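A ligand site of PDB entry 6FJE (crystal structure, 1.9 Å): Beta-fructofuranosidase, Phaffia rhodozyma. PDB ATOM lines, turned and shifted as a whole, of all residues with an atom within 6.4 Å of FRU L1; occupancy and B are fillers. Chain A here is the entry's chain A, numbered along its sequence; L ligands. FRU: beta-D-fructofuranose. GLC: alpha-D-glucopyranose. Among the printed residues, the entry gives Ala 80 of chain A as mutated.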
ATOM      1  N   TRP A  77      -0.895  -6.663  13.730  1.00  0.00           N
ATOM      2  CA  TRP A  77       0.384  -7.360  13.785  1.00  0.00           C
ATOM      3  C   TRP A  77       0.286  -8.749  13.173  1.00  0.00           C
ATOM      4  O   TRP A  77      -0.630  -9.505  13.499  1.00  0.00           O
ATOM      5  CB  TRP A  77       0.849  -7.504  15.241  1.00  0.00           C
ATOM      6  CG  TRP A  77       2.039  -8.376  15.374  1.00  0.00           C
ATOM      7  CD1 TRP A  77       2.042  -9.736  15.537  1.00  0.00           C
ATOM      8  CD2 TRP A  77       3.400  -7.972  15.307  1.00  0.00           C
ATOM      9  NE1 TRP A  77       3.328 -10.192  15.566  1.00  0.00           N
ATOM     10  CE2 TRP A  77       4.188  -9.127  15.434  1.00  0.00           C
ATOM     11  CE3 TRP A  77       4.043  -6.733  15.157  1.00  0.00           C
ATOM     12  CZ2 TRP A  77       5.576  -9.099  15.420  1.00  0.00           C
ATOM     13  CZ3 TRP A  77       5.421  -6.697  15.136  1.00  0.00           C
ATOM     14  CH2 TRP A  77       6.175  -7.866  15.265  1.00  0.00           C
ATOM     15  N   ASN A  79       3.274 -12.081  12.258  1.00  0.00           N
ATOM     16  CA  ASN A  79       4.615 -12.578  12.048  1.00  0.00           C
ATOM     17  C   ASN A  79       4.641 -13.917  11.288  1.00  0.00           C
ATOM     18  O   ASN A  79       4.194 -13.960  10.139  1.00  0.00           O
ATOM     19  CB  ASN A  79       5.545 -12.473  13.313  1.00  0.00           C
ATOM     20  CG  ASN A  79       5.034 -13.198  14.545  1.00  0.00           C
ATOM     21  OD1 ASN A  79       4.026 -12.841  15.137  1.00  0.00           O
ATOM     22  ND2 ASN A  79       5.818 -14.184  15.013  1.00  0.00           N
ATOM     23  N   ALA A  80       5.170 -14.970  11.888  1.00  0.00           N
ATOM     24  CA  ALA A  80       5.522 -16.192  11.187  1.00  0.00           C
ATOM     25  C   ALA A  80       4.352 -16.890  10.501  1.00  0.00           C
ATOM     26  O   ALA A  80       3.269 -16.991  11.068  1.00  0.00           O
ATOM     27  CB  ALA A  80       6.159 -17.180  12.157  1.00  0.00           C
ATOM     28  N   GLN A  97       0.938 -16.215  12.509  1.00  0.00           N
ATOM     29  CA  GLN A  97       0.938 -15.609  13.837  1.00  0.00           C
ATOM     30  C   GLN A  97       0.326 -14.206  13.736  1.00  0.00           C
ATOM     31  O   GLN A  97       0.802 -13.386  12.935  1.00  0.00           O
ATOM     32  CB  GLN A  97       2.362 -15.554  14.387  1.00  0.00           C
ATOM     33  CG  GLN A  97       2.966 -16.931  14.638  1.00  0.00           C
ATOM     34  CD  GLN A  97       2.524 -17.528  15.948  1.00  0.00           C
ATOM     35  OE1 GLN A  97       3.096 -17.218  16.993  1.00  0.00           O
ATOM     36  NE2 GLN A  97       1.499 -18.378  15.916  1.00  0.00           N
ATOM     37  N   TRP A 105       3.480  -7.588  18.990  1.00  0.00           N
ATOM     38  CA  TRP A 105       3.165  -8.984  19.279  1.00  0.00           C
ATOM     39  C   TRP A 105       2.414  -9.162  20.599  1.00  0.00           C
ATOM     40  O   TRP A 105       2.637  -8.427  21.567  1.00  0.00           O
ATOM     41  CB  TRP A 105       4.490  -9.760  19.307  1.00  0.00           C
ATOM     42  CG  TRP A 105       4.473 -11.248  19.521  1.00  0.00           C
ATOM     43  CD1 TRP A 105       4.578 -12.205  18.562  1.00  0.00           C
ATOM     44  CD2 TRP A 105       4.498 -11.926  20.772  1.00  0.00           C
ATOM     45  NE1 TRP A 105       4.615 -13.463  19.141  1.00  0.00           N
ATOM     46  CE2 TRP A 105       4.565 -13.317  20.498  1.00  0.00           C
ATOM     47  CE3 TRP A 105       4.462 -11.505  22.117  1.00  0.00           C
ATOM     48  CZ2 TRP A 105       4.606 -14.273  21.515  1.00  0.00           C
ATOM     49  CZ3 TRP A 105       4.491 -12.464  23.115  1.00  0.00           C
ATOM     50  CH2 TRP A 105       4.572 -13.827  22.812  1.00  0.00           C
ATOM     51  N   ILE A 108      -0.843 -14.299  20.964  1.00  0.00           N
ATOM     52  CA  ILE A 108      -0.569 -14.633  19.582  1.00  0.00           C
ATOM     53  C   ILE A 108      -1.453 -15.824  19.162  1.00  0.00           C
ATOM     54  O   ILE A 108      -1.657 -16.767  19.920  1.00  0.00           O
ATOM     55  CB  ILE A 108       0.943 -14.791  19.308  1.00  0.00           C
ATOM     56  CG1 ILE A 108       1.258 -14.513  17.827  1.00  0.00           C
ATOM     57  CG2 ILE A 108       1.445 -16.162  19.731  1.00  0.00           C
ATOM     58  CD1 ILE A 108       1.152 -13.039  17.435  1.00  0.00           C
ATOM     59  N   VAL A 144      -0.615 -19.077  21.224  1.00  0.00           N
ATOM     60  CA  VAL A 144      -0.606 -20.157  20.264  1.00  0.00           C
ATOM     61  C   VAL A 144       0.507 -19.857  19.278  1.00  0.00           C
ATOM     62  O   VAL A 144       0.334 -19.082  18.334  1.00  0.00           O
ATOM     63  CB  VAL A 144      -1.983 -20.286  19.556  1.00  0.00           C
ATOM     64  CG1 VAL A 144      -1.953 -21.347  18.466  1.00  0.00           C
ATOM     65  CG2 VAL A 144      -3.066 -20.631  20.564  1.00  0.00           C
ATOM     66  N   PHE A 145       1.659 -20.456  19.534  1.00  0.00           N
ATOM     67  CA  PHE A 145       2.868 -20.232  18.758  1.00  0.00           C
ATOM     68  C   PHE A 145       2.805 -21.074  17.468  1.00  0.00           C
ATOM     69  O   PHE A 145       1.766 -21.675  17.143  1.00  0.00           O
ATOM     70  CB  PHE A 145       4.116 -20.571  19.599  1.00  0.00           C
ATOM     71  CG  PHE A 145       4.576 -19.485  20.546  1.00  0.00           C
ATOM     72  CD1 PHE A 145       3.694 -18.620  21.182  1.00  0.00           C
ATOM     73  CD2 PHE A 145       5.916 -19.403  20.883  1.00  0.00           C
ATOM     74  CE1 PHE A 145       4.137 -17.673  22.086  1.00  0.00           C
ATOM     75  CE2 PHE A 145       6.372 -18.445  21.782  1.00  0.00           C
ATOM     76  CZ  PHE A 145       5.476 -17.585  22.386  1.00  0.00           C
ATOM     77  N   ASP A 146       3.907 -21.114  16.712  1.00  0.00           N
ATOM     78  CA  ASP A 146       3.986 -21.815  15.440  1.00  0.00           C
ATOM     79  C   ASP A 146       3.620 -23.305  15.577  1.00  0.00           C
ATOM     80  O   ASP A 146       3.821 -23.933  16.620  1.00  0.00           O
ATOM     81  CB  ASP A 146       5.416 -21.648  14.897  1.00  0.00           C
ATOM     82  CG  ASP A 146       5.633 -22.157  13.470  1.00  0.00           C
ATOM     83  OD1 ASP A 146       4.675 -22.332  12.693  1.00  0.00           O
ATOM     84  OD2 ASP A 146       6.841 -22.369  13.139  1.00  0.00           O
ATOM     85  N   GLY A 147       3.048 -23.831  14.503  1.00  0.00           N
ATOM     86  CA  GLY A 147       2.714 -25.244  14.384  1.00  0.00           C
ATOM     87  C   GLY A 147       2.635 -25.670  12.938  1.00  0.00           C
ATOM     88  O   GLY A 147       2.645 -24.838  12.030  1.00  0.00           O
ATOM     89  N   THR A 163       3.025 -25.125  19.250  1.00  0.00           N
ATOM     90  CA  THR A 163       3.562 -24.801  20.548  1.00  0.00           C
ATOM     91  C   THR A 163       2.529 -24.016  21.362  1.00  0.00           C
ATOM     92  O   THR A 163       2.139 -22.887  21.008  1.00  0.00           O
ATOM     93  CB  THR A 163       4.888 -24.040  20.446  1.00  0.00           C
ATOM     94  OG1 THR A 163       5.861 -24.874  19.809  1.00  0.00           O
ATOM     95  CG2 THR A 163       5.377 -23.642  21.829  1.00  0.00           C
ATOM     96  N   ARG A 220      10.216 -25.185  20.903  1.00  0.00           N
ATOM     97  CA  ARG A 220       9.058 -24.758  20.119  1.00  0.00           C
ATOM     98  C   ARG A 220       9.156 -25.053  18.643  1.00  0.00           C
ATOM     99  O   ARG A 220      10.186 -25.520  18.141  1.00  0.00           O
ATOM    100  CB  ARG A 220       8.789 -23.254  20.352  1.00  0.00           C
ATOM    101  CG  ARG A 220       9.918 -22.303  19.993  1.00  0.00           C
ATOM    102  CD  ARG A 220       9.456 -20.837  20.014  1.00  0.00           C
ATOM    103  NE  ARG A 220      10.578 -19.910  19.988  1.00  0.00           N
ATOM    104  CZ  ARG A 220      11.377 -19.624  21.028  1.00  0.00           C
ATOM    105  NH1 ARG A 220      11.165 -20.176  22.214  1.00  0.00           N
ATOM    106  NH2 ARG A 220      12.403 -18.793  20.881  1.00  0.00           N
ATOM    107  N   ASP A 221       8.029 -24.782  17.969  1.00  0.00           N
ATOM    108  CA  ASP A 221       7.907 -24.788  16.518  1.00  0.00           C
ATOM    109  C   ASP A 221       7.966 -26.203  15.951  1.00  0.00           C
ATOM    110  O   ASP A 221       8.835 -26.494  15.108  1.00  0.00           O
ATOM    111  CB  ASP A 221       8.938 -23.863  15.855  1.00  0.00           C
ATOM    112  CG  ASP A 221       8.910 -22.443  16.430  1.00  0.00           C
ATOM    113  OD1 ASP A 221       7.896 -22.064  17.042  1.00  0.00           O
ATOM    114  OD2 ASP A 221       9.938 -21.746  16.264  1.00  0.00           O
ATOM    115  N   PHE A 302      17.683 -22.187  17.889  1.00  0.00           N
ATOM    116  CA  PHE A 302      16.957 -22.309  16.616  1.00  0.00           C
ATOM    117  C   PHE A 302      15.470 -21.995  16.806  1.00  0.00           C
ATOM    118  O   PHE A 302      14.892 -22.261  17.872  1.00  0.00           O
ATOM    119  CB  PHE A 302      17.009 -23.735  16.045  1.00  0.00           C
ATOM    120  CG  PHE A 302      18.369 -24.182  15.534  1.00  0.00           C
ATOM    121  CD1 PHE A 302      19.299 -23.308  14.985  1.00  0.00           C
ATOM    122  CD2 PHE A 302      18.690 -25.536  15.584  1.00  0.00           C
ATOM    123  CE1 PHE A 302      20.529 -23.774  14.532  1.00  0.00           C
ATOM    124  CE2 PHE A 302      19.909 -26.016  15.112  1.00  0.00           C
ATOM    125  CZ  PHE A 302      20.826 -25.121  14.578  1.00  0.00           C
ATOM    126  N   GLU A 303      14.875 -21.468  15.746  1.00  0.00           N
ATOM    127  CA  GLU A 303      13.431 -21.274  15.632  1.00  0.00           C
ATOM    128  C   GLU A 303      12.956 -21.720  14.259  1.00  0.00           C
ATOM    129  O   GLU A 303      13.715 -21.695  13.285  1.00  0.00           O
ATOM    130  CB  GLU A 303      13.035 -19.806  15.865  1.00  0.00           C
ATOM    131  CG  GLU A 303      13.391 -19.253  17.239  1.00  0.00           C
ATOM    132  CD  GLU A 303      12.983 -17.805  17.404  1.00  0.00           C
ATOM    133  OE1 GLU A 303      13.455 -16.951  16.635  1.00  0.00           O
ATOM    134  OE2 GLU A 303      12.196 -17.514  18.326  1.00  0.00           O
ATOM    135  N   THR A 304      11.677 -22.118  14.200  1.00  0.00           N
ATOM    136  CA  THR A 304      10.971 -22.496  12.973  1.00  0.00           C
ATOM    137  C   THR A 304      11.751 -23.435  12.054  1.00  0.00           C
ATOM    138  O   THR A 304      11.679 -23.307  10.836  1.00  0.00           O
ATOM    139  CB  THR A 304      10.435 -21.262  12.182  1.00  0.00           C
ATOM    140  OG1 THR A 304      11.483 -20.618  11.431  1.00  0.00           O
ATOM    141  CG2 THR A 304       9.771 -20.247  13.104  1.00  0.00           C
ATOM    142  N   GLU A 334      18.942 -17.232  16.391  1.00  0.00           N
ATOM    143  CA  GLU A 334      18.924 -15.960  17.086  1.00  0.00           C
ATOM    144  C   GLU A 334      20.197 -15.682  17.889  1.00  0.00           C
ATOM    145  O   GLU A 334      20.891 -16.593  18.307  1.00  0.00           O
ATOM    146  CB  GLU A 334      17.685 -15.773  17.950  1.00  0.00           C
ATOM    147  CG  GLU A 334      17.230 -16.920  18.800  1.00  0.00           C
ATOM    148  CD  GLU A 334      15.860 -16.651  19.453  1.00  0.00           C
ATOM    149  OE1 GLU A 334      15.198 -15.632  19.138  1.00  0.00           O
ATOM    150  OE2 GLU A 334      15.447 -17.482  20.273  1.00  0.00           O
ATOM    151  N   HIS A 343      18.521 -11.991  13.875  1.00  0.00           N
ATOM    152  CA  HIS A 343      17.915 -13.180  13.255  1.00  0.00           C
ATOM    153  C   HIS A 343      18.481 -13.528  11.875  1.00  0.00           C
ATOM    154  O   HIS A 343      18.457 -12.689  10.980  1.00  0.00           O
ATOM    155  CB  HIS A 343      16.411 -12.956  13.112  1.00  0.00           C
ATOM    156  CG  HIS A 343      15.634 -13.154  14.367  1.00  0.00           C
ATOM    157  ND1 HIS A 343      14.423 -12.538  14.600  1.00  0.00           N
ATOM    158  CD2 HIS A 343      15.902 -13.889  15.469  1.00  0.00           C
ATOM    159  CE1 HIS A 343      13.967 -12.897  15.785  1.00  0.00           C
ATOM    160  NE2 HIS A 343      14.842 -13.719  16.344  1.00  0.00           N
ATOM    161  N   TYR A 376      12.438 -13.723   7.953  1.00  0.00           N
ATOM    162  CA  TYR A 376      12.682 -14.722   8.987  1.00  0.00           C
ATOM    163  C   TYR A 376      11.493 -15.666   9.029  1.00  0.00           C
ATOM    164  O   TYR A 376      10.464 -15.386   8.407  1.00  0.00           O
ATOM    165  CB  TYR A 376      12.831 -14.035  10.340  1.00  0.00           C
ATOM    166  CG  TYR A 376      13.417 -14.872  11.452  1.00  0.00           C
ATOM    167  CD1 TYR A 376      14.677 -15.449  11.335  1.00  0.00           C
ATOM    168  CD2 TYR A 376      12.707 -15.079  12.644  1.00  0.00           C
ATOM    169  CE1 TYR A 376      15.228 -16.198  12.361  1.00  0.00           C
ATOM    170  CE2 TYR A 376      13.254 -15.837  13.680  1.00  0.00           C
ATOM    171  CZ  TYR A 376      14.514 -16.387  13.538  1.00  0.00           C
ATOM    172  OH  TYR A 376      15.086 -17.145  14.554  1.00  0.00           O
ATOM    173  N   ALA A 377      11.641 -16.771   9.762  1.00  0.00           N
ATOM    174  CA  ALA A 377      10.542 -17.673  10.079  1.00  0.00           C
ATOM    175  C   ALA A 377      10.009 -18.344   8.842  1.00  0.00           C
ATOM    176  O   ALA A 377       8.807 -18.406   8.621  1.00  0.00           O
ATOM    177  CB  ALA A 377       9.440 -16.942  10.849  1.00  0.00           C
ATOM    178  N   TRP A 393       8.357 -14.554   6.583  1.00  0.00           N
ATOM    179  CA  TRP A 393       7.789 -13.302   7.069  1.00  0.00           C
ATOM    180  C   TRP A 393       8.788 -12.171   6.835  1.00  0.00           C
ATOM    181  O   TRP A 393       9.951 -12.297   7.228  1.00  0.00           O
ATOM    182  CB  TRP A 393       7.484 -13.457   8.553  1.00  0.00           C
ATOM    183  CG  TRP A 393       7.393 -12.217   9.405  1.00  0.00           C
ATOM    184  CD1 TRP A 393       6.551 -11.173   9.245  1.00  0.00           C
ATOM    185  CD2 TRP A 393       8.121 -11.972  10.603  1.00  0.00           C
ATOM    186  NE1 TRP A 393       6.728 -10.258  10.249  1.00  0.00           N
ATOM    187  CE2 TRP A 393       7.687 -10.722  11.106  1.00  0.00           C
ATOM    188  CE3 TRP A 393       9.108 -12.673  11.305  1.00  0.00           C
ATOM    189  CZ2 TRP A 393       8.204 -10.172  12.274  1.00  0.00           C
ATOM    190  CZ3 TRP A 393       9.624 -12.123  12.473  1.00  0.00           C
ATOM    191  CH2 TRP A 393       9.177 -10.879  12.943  1.00  0.00           C
HETATM  192  C1  FRU L   1       9.805 -16.905  15.105  1.00  0.00           C
HETATM  193  C2  FRU L   1       8.926 -17.181  16.318  1.00  0.00           C
HETATM  194  C3  FRU L   1       8.710 -18.662  16.556  1.00  0.00           C
HETATM  195  C4  FRU L   1       7.495 -18.619  17.464  1.00  0.00           C
HETATM  196  C5  FRU L   1       6.707 -17.405  16.951  1.00  0.00           C
HETATM  197  C6  FRU L   1       5.946 -16.696  18.057  1.00  0.00           C
HETATM  198  O1  FRU L   1       9.859 -15.488  14.930  1.00  0.00           O
HETATM  199  O2  FRU L   1       9.557 -16.611  17.454  1.00  0.00           O
HETATM  200  O3  FRU L   1       9.860 -19.317  17.125  1.00  0.00           O
HETATM  201  O4  FRU L   1       6.712 -19.809  17.387  1.00  0.00           O
HETATM  202  O5  FRU L   1       7.630 -16.532  16.302  1.00  0.00           O
HETATM  203  O6  FRU L   1       5.046 -15.689  17.536  1.00  0.00           O
HETATM  204  C1  GLC L   2       8.591 -14.260  19.409  1.00  0.00           C
HETATM  205  C2  GLC L   2       8.436 -13.508  20.761  1.00  0.00           C
HETATM  206  C3  GLC L   2       9.426 -13.971  21.867  1.00  0.00           C
HETATM  207  C4  GLC L   2      10.644 -14.779  21.368  1.00  0.00           C
HETATM  208  C5  GLC L   2      10.966 -14.279  19.957  1.00  0.00           C
HETATM  209  C6  GLC L   2      12.294 -14.702  19.340  1.00  0.00           C
HETATM  210  O1  GLC L   2       8.255 -13.479  18.248  1.00  0.00           O
HETATM  211  O2  GLC L   2       8.505 -12.079  20.596  1.00  0.00           O
HETATM  212  O3  GLC L   2       8.691 -14.769  22.796  1.00  0.00           O
HETATM  213  O4  GLC L   2      11.791 -14.680  22.249  1.00  0.00           O
HETATM  214  O5  GLC L   2       9.896 -14.804  19.177  1.00  0.00           O
HETATM  215  O6  GLC L   2      12.102 -14.775  17.905  1.00  0.00           O
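OE2 of Glu 303 is in hydrogen-bond range of O2 of FRU L1 (2.9 Å).
OD1 of Asp 221 sits at hydrogen-bond distance from O4 of FRU L1 (2.6 Å).
The side-chain carboxylate of Glu 334 sits close to an oxygen (O6) of GLC L2 (3.4 Å).
O6 of GLC L2 is in hydrogen-bond range of OE2 of Glu 303 (2.8 Å).
NE of Arg 220 is in hydrogen-bond range of O3 of FRU L1 (3.0 Å).
NE1 of Trp 105 is in hydrogen-bond range of O6 of FRU L1 (2.8 Å).
The side-chain amide oxygen of Gln 97 sits at hydrogen-bond distance from an oxygen (O6) of FRU L1, at 2.5 Å.
N of Asp 146 lies within hydrogen-bond range of O4 of FRU L1 (3.2 Å).
NE2 of His 343 sits at hydrogen-bond distance from O6 of GLC L2 (3.3 Å).
An oxygen (O6) of FRU L1 lies within hydrogen-bond range of the side-chain amide nitrogen (ND2) of Asn 79, at 3.0 Å.
O5 of GLC L2 lies within hydrogen-bond range of O2 of FRU L1 (2.5 Å).
N of Thr 304 is in hydrogen-bond range of OD2 of Asp 221 (2.7 Å).
The side-chain carboxylate (OE2) of Glu 303 is in salt-bridge range of the guanidinium group (NH2) of Arg 220 (2.9 Å).
N of Asn 79 lies within hydrogen-bond range of O of Gln 97, at 2.9 Å.
The indole nitrogen (NE1) of Trp 77 is in hydrogen-bond range of the side-chain amide oxygen (OD1) of Asn 79.
The guanidinium group of Arg 220 lies within salt-bridge range of the side-chain carboxylate of Glu 334.
The side-chain hydroxyl (OG1) of Thr 163 lies within hydrogen-bond range of the backbone NH (N) of Asp 221 (2.8 Å).
The backbone NH (N) of Val 144 is in hydrogen-bond range of the backbone carbonyl oxygen (O) of Ile 108, at 2.8 Å.
O of Ala 80 lies within hydrogen-bond range of N of Gln 97 (2.8 Å).
Residues that only touch FRU L1: Ile 108 (3.98 Å), Phe 145 (3.5 Å), Thr 304 (3.9 Å) and Tyr 376 (3.6 Å).
Hydrophobic or aromatic side chains that line FRU L1: Trp 105, Ile 108, Phe 145 and Tyr 376.
Of the 21 residues printed, 11 come within 4 Å of FRU L1.
The nearest printed residue that does not touch FRU L1 is Trp 393 (4.2 Å).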
